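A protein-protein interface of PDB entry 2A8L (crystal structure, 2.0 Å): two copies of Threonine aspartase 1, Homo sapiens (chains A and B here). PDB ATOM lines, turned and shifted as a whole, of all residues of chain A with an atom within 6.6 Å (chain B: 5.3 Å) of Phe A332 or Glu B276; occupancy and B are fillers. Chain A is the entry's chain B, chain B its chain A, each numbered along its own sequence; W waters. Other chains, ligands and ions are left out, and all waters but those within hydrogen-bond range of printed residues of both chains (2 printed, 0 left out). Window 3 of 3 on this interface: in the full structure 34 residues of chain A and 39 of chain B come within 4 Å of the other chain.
The backbone NH (N) of Ala B275 is in hydrogen-bond range of the side-chain sulfur (SD) of Met B120 (3.5 Å).
NE1 of Trp B274 is in hydrogen-bond range of OE1 of Glu B276, at 2.9 Å.
The backbone carbonyl oxygen (O) of Glu B276 sits close to the side-chain amide oxygen (OD1) of Asn B282, 3.3 Å away.
The backbone carbonyl oxygen (O) of Glu B276 is in hydrogen-bond range of the backbone NH (N) of Thr B286 (2.9 Å).
N of Phe A332 sits close to OG of Ser A330 (3.2 Å).
The side-chain hydroxyl (OH) of Tyr B269 sits at hydrogen-bond distance from the backbone carbonyl oxygen (O) of Arg A299 (2.9 Å).
Arg A299 touches Leu B125 (NH1 to O, 3.5 Å).
Leu B125 touches Pro A331.
Phe A332 touches Met B120 (CE2 to CE, 3.8 Å).
CD2 of Phe A332 touches CD1 of Leu B125, 3.7 Å away.
Tyr B269 touches Phe A332.
Phe A332 touches Trp B274 (CZ to CZ2, 3.5 Å).
Phe A332 touches Glu B276.
Of the printed residues of chain B, Arg A299 touches Leu B125 (3.5 Å) and Tyr B269 (2.9 Å).
Phe A332 touches five residues of chain B.
Of the printed residues of chain A, Trp B274 touches Phe A332.
Glu B276 touches just one residue of chain A: Phe A332.
Thr B278 touches none of the printed residues of chain A.
Ser B285 touches none of the printed residues of chain A.
The nearest residue of chain A that does not touch Glu B276 is Pro A331 (6.4 Å).
Hydrophobic or aromatic side chains of chain A that line the printed part of chain B: Phe A332.
Of the 18 printed residues of chain B, 5 touch a printed residue of chain A.
Hydrophobic or aromatic side chains of chain B that line the printed part of chain A: Met B120, Leu B125, Tyr B269 and Trp B274.
Among the printed residues, 8 pairs touch across the chains.
Among the printed residues, no Asp or Glu carboxylate lies within 4 Å of a Lys or Arg side-chain nitrogen of the other chain.
Water W1 bridges O of Phe A332 (2.6 Å) and O of Leu B125 (3.2 Å).
Water W2 lies within hydrogen-bond range of OH of Tyr B269 (2.7 Å), O of Leu B125 (2.9 Å) and NH1 of Arg A299 (2.9 Å).
No position is printed for both chains.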
ATOM      1  N   ARG A 299     -25.511  -9.863  20.783  1.00  0.00           N
ATOM      2  CA  ARG A 299     -24.713  -9.926  22.007  1.00  0.00           C
ATOM      3  C   ARG A 299     -24.719 -11.329  22.603  1.00  0.00           C
ATOM      4  O   ARG A 299     -23.756 -11.745  23.259  1.00  0.00           O
ATOM      5  CB  ARG A 299     -25.253  -8.930  23.040  1.00  0.00           C
ATOM      6  CG  ARG A 299     -25.370  -7.494  22.542  1.00  0.00           C
ATOM      7  CD  ARG A 299     -24.023  -6.822  22.431  1.00  0.00           C
ATOM      8  NE  ARG A 299     -24.153  -5.378  22.246  1.00  0.00           N
ATOM      9  CZ  ARG A 299     -23.226  -4.495  22.605  1.00  0.00           C
ATOM     10  NH1 ARG A 299     -22.100  -4.907  23.172  1.00  0.00           N
ATOM     11  NH2 ARG A 299     -23.426  -3.199  22.402  1.00  0.00           N
ATOM     12  N   THR A 300     -25.804 -12.059  22.373  1.00  0.00           N
ATOM     13  CA  THR A 300     -25.925 -13.413  22.898  1.00  0.00           C
ATOM     14  C   THR A 300     -25.656 -14.517  21.867  1.00  0.00           C
ATOM     15  O   THR A 300     -25.663 -15.699  22.216  1.00  0.00           O
ATOM     16  CB  THR A 300     -27.333 -13.636  23.523  1.00  0.00           C
ATOM     17  OG1 THR A 300     -28.352 -13.307  22.570  1.00  0.00           O
ATOM     18  CG2 THR A 300     -27.513 -12.761  24.751  1.00  0.00           C
ATOM     19  N   SER A 329     -31.689 -13.543  30.986  1.00  0.00           N
ATOM     20  CA  SER A 329     -30.777 -13.318  32.097  1.00  0.00           C
ATOM     21  C   SER A 329     -29.298 -13.289  31.754  1.00  0.00           C
ATOM     22  O   SER A 329     -28.458 -13.339  32.648  1.00  0.00           O
ATOM     23  CB  SER A 329     -31.028 -14.365  33.184  1.00  0.00           C
ATOM     24  OG  SER A 329     -32.364 -14.278  33.651  1.00  0.00           O
ATOM     25  N   SER A 330     -28.967 -13.204  30.471  1.00  0.00           N
ATOM     26  CA  SER A 330     -27.565 -13.161  30.083  1.00  0.00           C
ATOM     27  C   SER A 330     -26.878 -11.907  30.626  1.00  0.00           C
ATOM     28  O   SER A 330     -27.431 -10.808  30.561  1.00  0.00           O
ATOM     29  CB  SER A 330     -27.423 -13.188  28.564  1.00  0.00           C
ATOM     30  OG  SER A 330     -26.080 -12.922  28.201  1.00  0.00           O
ATOM     31  N   PRO A 331     -25.664 -12.062  31.182  1.00  0.00           N
ATOM     32  CA  PRO A 331     -24.893 -10.940  31.734  1.00  0.00           C
ATOM     33  C   PRO A 331     -24.603  -9.908  30.646  1.00  0.00           C
ATOM     34  O   PRO A 331     -24.375  -8.730  30.930  1.00  0.00           O
ATOM     35  CB  PRO A 331     -23.614 -11.612  32.229  1.00  0.00           C
ATOM     36  CG  PRO A 331     -24.077 -12.992  32.590  1.00  0.00           C
ATOM     37  CD  PRO A 331     -24.988 -13.344  31.446  1.00  0.00           C
ATOM     38  N   PHE A 332     -24.612 -10.363  29.396  1.00  0.00           N
ATOM     39  CA  PHE A 332     -24.355  -9.483  28.265  1.00  0.00           C
ATOM     40  C   PHE A 332     -25.507  -8.538  27.950  1.00  0.00           C
ATOM     41  O   PHE A 332     -25.373  -7.660  27.101  1.00  0.00           O
ATOM     42  CB  PHE A 332     -23.993 -10.306  27.022  1.00  0.00           C
ATOM     43  CG  PHE A 332     -22.677 -11.028  27.142  1.00  0.00           C
ATOM     44  CD1 PHE A 332     -22.585 -12.229  27.837  1.00  0.00           C
ATOM     45  CD2 PHE A 332     -21.519 -10.476  26.601  1.00  0.00           C
ATOM     46  CE1 PHE A 332     -21.357 -12.871  27.998  1.00  0.00           C
ATOM     47  CE2 PHE A 332     -20.289 -11.105  26.755  1.00  0.00           C
ATOM     48  CZ  PHE A 332     -20.206 -12.305  27.456  1.00  0.00           C
ATOM     49  N   LEU A 333     -26.640  -8.717  28.625  1.00  0.00           N
ATOM     50  CA  LEU A 333     -27.801  -7.850  28.415  1.00  0.00           C
ATOM     51  C   LEU A 333     -28.341  -7.329  29.754  1.00  0.00           C
ATOM     52  O   LEU A 333     -29.434  -6.768  29.817  1.00  0.00           O
ATOM     53  CB  LEU A 333     -28.917  -8.612  27.682  1.00  0.00           C
ATOM     54  CG  LEU A 333     -28.615  -9.094  26.257  1.00  0.00           C
ATOM     55  CD1 LEU A 333     -29.814  -9.862  25.709  1.00  0.00           C
ATOM     56  CD2 LEU A 333     -28.276  -7.902  25.365  1.00  0.00           C
ATOM     57  N   ALA A 334     -27.562  -7.524  30.815  1.00  0.00           N
ATOM     58  CA  ALA A 334     -27.954  -7.112  32.160  1.00  0.00           C
ATOM     59  C   ALA A 334     -28.396  -5.660  32.264  1.00  0.00           C
ATOM     60  O   ALA A 334     -29.281  -5.332  33.054  1.00  0.00           O
ATOM     61  CB  ALA A 334     -26.808  -7.372  33.134  1.00  0.00           C
ATOM     62  N   SER A 335     -27.786  -4.790  31.471  1.00  0.00           N
ATOM     63  CA  SER A 335     -28.133  -3.377  31.516  1.00  0.00           C
ATOM     64  C   SER A 335     -29.416  -3.051  30.761  1.00  0.00           C
ATOM     65  O   SER A 335     -29.933  -1.939  30.868  1.00  0.00           O
ATOM     66  CB  SER A 335     -26.985  -2.540  30.956  1.00  0.00           C
ATOM     67  OG  SER A 335     -25.817  -2.706  31.737  1.00  0.00           O
ATOM     68  N   GLU A 336     -29.930  -4.011  30.001  1.00  0.00           N
ATOM     69  CA  GLU A 336     -31.151  -3.780  29.237  1.00  0.00           C
ATOM     70  C   GLU A 336     -32.414  -3.990  30.057  1.00  0.00           C
ATOM     71  O   GLU A 336     -32.523  -4.944  30.827  1.00  0.00           O
ATOM     72  CB  GLU A 336     -31.197  -4.690  28.005  1.00  0.00           C
ATOM     73  CG  GLU A 336     -30.116  -4.394  26.984  1.00  0.00           C
ATOM     74  CD  GLU A 336     -30.092  -2.933  26.589  1.00  0.00           C
ATOM     75  OE1 GLU A 336     -31.130  -2.434  26.106  1.00  0.00           O
ATOM     76  OE2 GLU A 336     -29.036  -2.284  26.766  1.00  0.00           O
ATOM     77  N   MET B 120     -13.687  -4.725  22.162  1.00  0.00           N
ATOM     78  CA  MET B 120     -14.613  -5.170  23.194  1.00  0.00           C
ATOM     79  C   MET B 120     -14.055  -4.860  24.578  1.00  0.00           C
ATOM     80  O   MET B 120     -12.857  -4.995  24.831  1.00  0.00           O
ATOM     81  CB  MET B 120     -14.887  -6.678  23.049  1.00  0.00           C
ATOM     82  CG  MET B 120     -16.025  -7.207  23.920  1.00  0.00           C
ATOM     83  SD  MET B 120     -16.513  -8.867  23.401  1.00  0.00           S
ATOM     84  CE  MET B 120     -17.848  -9.219  24.560  1.00  0.00           C
ATOM     85  N   ASP B 121     -14.939  -4.433  25.467  1.00  0.00           N
ATOM     86  CA  ASP B 121     -14.548  -4.081  26.825  1.00  0.00           C
ATOM     87  C   ASP B 121     -14.981  -5.148  27.821  1.00  0.00           C
ATOM     88  O   ASP B 121     -16.164  -5.420  27.966  1.00  0.00           O
ATOM     89  CB  ASP B 121     -15.168  -2.737  27.213  1.00  0.00           C
ATOM     90  CG  ASP B 121     -14.787  -2.307  28.619  1.00  0.00           C
ATOM     91  OD1 ASP B 121     -13.577  -2.263  28.923  1.00  0.00           O
ATOM     92  OD2 ASP B 121     -15.699  -2.010  29.416  1.00  0.00           O
ATOM     93  N   GLY B 122     -14.014  -5.724  28.526  1.00  0.00           N
ATOM     94  CA  GLY B 122     -14.326  -6.764  29.491  1.00  0.00           C
ATOM     95  C   GLY B 122     -15.181  -6.331  30.675  1.00  0.00           C
ATOM     96  O   GLY B 122     -16.001  -7.108  31.168  1.00  0.00           O
ATOM     97  N   LEU B 125     -18.674  -5.235  28.929  1.00  0.00           N
ATOM     98  CA  LEU B 125     -19.052  -6.219  27.914  1.00  0.00           C
ATOM     99  C   LEU B 125     -19.565  -5.543  26.650  1.00  0.00           C
ATOM    100  O   LEU B 125     -20.103  -6.206  25.767  1.00  0.00           O
ATOM    101  CB  LEU B 125     -20.130  -7.181  28.433  1.00  0.00           C
ATOM    102  CG  LEU B 125     -19.780  -7.989  29.683  1.00  0.00           C
ATOM    103  CD1 LEU B 125     -20.913  -8.966  29.960  1.00  0.00           C
ATOM    104  CD2 LEU B 125     -18.460  -8.728  29.485  1.00  0.00           C
ATOM    105  N   VAL B 246     -10.047  -6.067  31.504  1.00  0.00           N
ATOM    106  CA  VAL B 246      -9.422  -6.457  30.249  1.00  0.00           C
ATOM    107  C   VAL B 246     -10.167  -5.880  29.043  1.00  0.00           C
ATOM    108  O   VAL B 246     -11.363  -5.609  29.115  1.00  0.00           O
ATOM    109  CB  VAL B 246      -9.346  -8.011  30.126  1.00  0.00           C
ATOM    110  CG1 VAL B 246      -8.556  -8.584  31.292  1.00  0.00           C
ATOM    111  CG2 VAL B 246     -10.736  -8.607  30.099  1.00  0.00           C
ATOM    112  N   TYR B 269     -18.646  -9.749  15.764  1.00  0.00           N
ATOM    113  CA  TYR B 269     -18.731 -10.067  17.178  1.00  0.00           C
ATOM    114  C   TYR B 269     -18.382 -11.542  17.397  1.00  0.00           C
ATOM    115  O   TYR B 269     -18.820 -12.411  16.630  1.00  0.00           O
ATOM    116  CB  TYR B 269     -20.161  -9.799  17.643  1.00  0.00           C
ATOM    117  CG  TYR B 269     -20.403  -9.946  19.125  1.00  0.00           C
ATOM    118  CD1 TYR B 269     -19.899  -9.010  20.030  1.00  0.00           C
ATOM    119  CD2 TYR B 269     -21.185 -10.992  19.618  1.00  0.00           C
ATOM    120  CE1 TYR B 269     -20.173  -9.107  21.387  1.00  0.00           C
ATOM    121  CE2 TYR B 269     -21.466 -11.100  20.978  1.00  0.00           C
ATOM    122  CZ  TYR B 269     -20.959 -10.151  21.855  1.00  0.00           C
ATOM    123  OH  TYR B 269     -21.268 -10.225  23.189  1.00  0.00           O
ATOM    124  N   TRP B 274     -12.396 -10.666  21.668  1.00  0.00           N
ATOM    125  CA  TRP B 274     -13.289 -10.916  22.798  1.00  0.00           C
ATOM    126  C   TRP B 274     -12.652 -10.354  24.069  1.00  0.00           C
ATOM    127  O   TRP B 274     -11.421 -10.376  24.235  1.00  0.00           O
ATOM    128  CB  TRP B 274     -13.551 -12.425  22.972  1.00  0.00           C
ATOM    129  CG  TRP B 274     -14.751 -12.739  23.854  1.00  0.00           C
ATOM    130  CD1 TRP B 274     -14.737 -13.167  25.156  1.00  0.00           C
ATOM    131  CD2 TRP B 274     -16.127 -12.648  23.479  1.00  0.00           C
ATOM    132  NE1 TRP B 274     -16.024 -13.349  25.611  1.00  0.00           N
ATOM    133  CE2 TRP B 274     -16.897 -13.039  24.599  1.00  0.00           C
ATOM    134  CE3 TRP B 274     -16.790 -12.273  22.300  1.00  0.00           C
ATOM    135  CZ2 TRP B 274     -18.293 -13.067  24.579  1.00  0.00           C
ATOM    136  CZ3 TRP B 274     -18.184 -12.303  22.278  1.00  0.00           C
ATOM    137  CH2 TRP B 274     -18.917 -12.698  23.413  1.00  0.00           C
ATOM    138  N   ALA B 275     -13.493  -9.833  24.954  1.00  0.00           N
ATOM    139  CA  ALA B 275     -13.046  -9.278  26.225  1.00  0.00           C
ATOM    140  C   ALA B 275     -14.177  -9.519  27.225  1.00  0.00           C
ATOM    141  O   ALA B 275     -15.310  -9.098  27.002  1.00  0.00           O
ATOM    142  CB  ALA B 275     -12.753  -7.769  26.082  1.00  0.00           C
ATOM    143  N   GLU B 276     -13.868 -10.196  28.326  1.00  0.00           N
ATOM    144  CA  GLU B 276     -14.882 -10.512  29.328  1.00  0.00           C
ATOM    145  C   GLU B 276     -14.242 -10.631  30.708  1.00  0.00           C
ATOM    146  O   GLU B 276     -13.410 -11.513  30.934  1.00  0.00           O
ATOM    147  CB  GLU B 276     -15.566 -11.832  28.944  1.00  0.00           C
ATOM    148  CG  GLU B 276     -16.714 -12.268  29.836  1.00  0.00           C
ATOM    149  CD  GLU B 276     -17.326 -13.595  29.387  1.00  0.00           C
ATOM    150  OE1 GLU B 276     -16.968 -14.093  28.290  1.00  0.00           O
ATOM    151  OE2 GLU B 276     -18.170 -14.140  30.133  1.00  0.00           O
ATOM    152  N   ASN B 277     -14.616  -9.734  31.621  1.00  0.00           N
ATOM    153  CA  ASN B 277     -14.071  -9.759  32.976  1.00  0.00           C
ATOM    154  C   ASN B 277     -14.591 -10.981  33.733  1.00  0.00           C
ATOM    155  O   ASN B 277     -15.560 -11.618  33.319  1.00  0.00           O
ATOM    156  CB  ASN B 277     -14.467  -8.496  33.754  1.00  0.00           C
ATOM    157  CG  ASN B 277     -13.527  -7.316  33.508  1.00  0.00           C
ATOM    158  OD1 ASN B 277     -13.615  -6.288  34.189  1.00  0.00           O
ATOM    159  ND2 ASN B 277     -12.631  -7.456  32.540  1.00  0.00           N
ATOM    160  N   THR B 278     -13.936 -11.314  34.839  1.00  0.00           N
ATOM    161  CA  THR B 278     -14.374 -12.443  35.650  1.00  0.00           C
ATOM    162  C   THR B 278     -15.841 -12.250  36.038  1.00  0.00           C
ATOM    163  O   THR B 278     -16.286 -11.122  36.280  1.00  0.00           O
ATOM    164  CB  THR B 278     -13.532 -12.563  36.934  1.00  0.00           C
ATOM    165  OG1 THR B 278     -12.156 -12.773  36.581  1.00  0.00           O
ATOM    166  CG2 THR B 278     -14.013 -13.731  37.783  1.00  0.00           C
ATOM    167  N   ASN B 282     -17.590 -17.105  34.726  1.00  0.00           N
ATOM    168  CA  ASN B 282     -16.385 -16.729  33.990  1.00  0.00           C
ATOM    169  C   ASN B 282     -15.276 -16.479  35.017  1.00  0.00           C
ATOM    170  O   ASN B 282     -14.972 -15.338  35.355  1.00  0.00           O
ATOM    171  CB  ASN B 282     -16.673 -15.464  33.168  1.00  0.00           C
ATOM    172  CG  ASN B 282     -15.690 -15.261  32.027  1.00  0.00           C
ATOM    173  OD1 ASN B 282     -14.980 -14.255  31.976  1.00  0.00           O
ATOM    174  ND2 ASN B 282     -15.648 -16.216  31.101  1.00  0.00           N
ATOM    175  N   TYR B 284     -12.019 -16.464  35.004  1.00  0.00           N
ATOM    176  CA  TYR B 284     -10.917 -15.588  34.643  1.00  0.00           C
ATOM    177  C   TYR B 284     -11.359 -14.457  33.723  1.00  0.00           C
ATOM    178  O   TYR B 284     -12.292 -14.612  32.936  1.00  0.00           O
ATOM    179  CB  TYR B 284      -9.833 -16.396  33.929  1.00  0.00           C
ATOM    180  CG  TYR B 284      -9.079 -17.383  34.794  1.00  0.00           C
ATOM    181  CD1 TYR B 284      -8.009 -16.968  35.587  1.00  0.00           C
ATOM    182  CD2 TYR B 284      -9.413 -18.739  34.797  1.00  0.00           C
ATOM    183  CE1 TYR B 284      -7.285 -17.876  36.356  1.00  0.00           C
ATOM    184  CE2 TYR B 284      -8.695 -19.658  35.565  1.00  0.00           C
ATOM    185  CZ  TYR B 284      -7.633 -19.219  36.339  1.00  0.00           C
ATOM    186  OH  TYR B 284      -6.909 -20.117  37.094  1.00  0.00           O
ATOM    187  N   SER B 285     -10.693 -13.312  33.830  1.00  0.00           N
ATOM    188  CA  SER B 285     -10.992 -12.203  32.939  1.00  0.00           C
ATOM    189  C   SER B 285     -10.159 -12.563  31.710  1.00  0.00           C
ATOM    190  O   SER B 285      -8.942 -12.706  31.811  1.00  0.00           O
ATOM    191  CB  SER B 285     -10.516 -10.878  33.546  1.00  0.00           C
ATOM    192  OG  SER B 285     -11.241 -10.556  34.724  1.00  0.00           O
ATOM    193  N   THR B 286     -10.799 -12.740  30.559  1.00  0.00           N
ATOM    194  CA  THR B 286     -10.053 -13.106  29.356  1.00  0.00           C
ATOM    195  C   THR B 286     -10.185 -12.098  28.225  1.00  0.00           C
ATOM    196  O   THR B 286     -11.201 -11.427  28.092  1.00  0.00           O
ATOM    197  CB  THR B 286     -10.497 -14.483  28.815  1.00  0.00           C
ATOM    198  OG1 THR B 286     -11.837 -14.387  28.314  1.00  0.00           O
ATOM    199  CG2 THR B 286     -10.456 -15.527  29.924  1.00  0.00           C
ATOM    200  N   ALA B 287      -9.144 -12.011  27.408  1.00  0.00           N
ATOM    201  CA  ALA B 287      -9.129 -11.102  26.267  1.00  0.00           C
ATOM    202  C   ALA B 287      -8.486 -11.875  25.129  1.00  0.00           C
ATOM    203  O   ALA B 287      -7.461 -12.538  25.322  1.00  0.00           O
ATOM    204  CB  ALA B 287      -8.317  -9.850  26.585  1.00  0.00           C
ATOM    205  N   ARG B 304     -14.278 -16.001  20.595  1.00  0.00           N
ATOM    206  CA  ARG B 304     -15.123 -16.409  21.715  1.00  0.00           C
ATOM    207  C   ARG B 304     -14.820 -17.833  22.151  1.00  0.00           C
ATOM    208  O   ARG B 304     -14.848 -18.143  23.341  1.00  0.00           O
ATOM    209  CB  ARG B 304     -16.608 -16.313  21.362  1.00  0.00           C
ATOM    210  CG  ARG B 304     -17.481 -16.843  22.505  1.00  0.00           C
ATOM    211  CD  ARG B 304     -18.962 -16.638  22.287  1.00  0.00           C
ATOM    212  NE  ARG B 304     -19.561 -15.910  23.407  1.00  0.00           N
ATOM    213  CZ  ARG B 304     -20.868 -15.866  23.661  1.00  0.00           C
ATOM    214  NH1 ARG B 304     -21.715 -16.520  22.876  1.00  0.00           N
ATOM    215  NH2 ARG B 304     -21.330 -15.155  24.687  1.00  0.00           N
ATOM    216  N   SER B 307     -11.882 -17.870  24.356  1.00  0.00           N
ATOM    217  CA  SER B 307     -12.215 -17.352  25.681  1.00  0.00           C
ATOM    218  C   SER B 307     -12.935 -18.412  26.520  1.00  0.00           C
ATOM    219  O   SER B 307     -12.686 -18.545  27.719  1.00  0.00           O
ATOM    220  CB  SER B 307     -13.094 -16.107  25.559  1.00  0.00           C
ATOM    221  OG  SER B 307     -13.304 -15.527  26.835  1.00  0.00           O
HETATM  222  O   HOH W   1     -23.246  -6.450  26.144  1.00  0.00           O
HETATM  223  O   HOH W   2     -21.638  -7.677  23.842  1.00  0.00           O
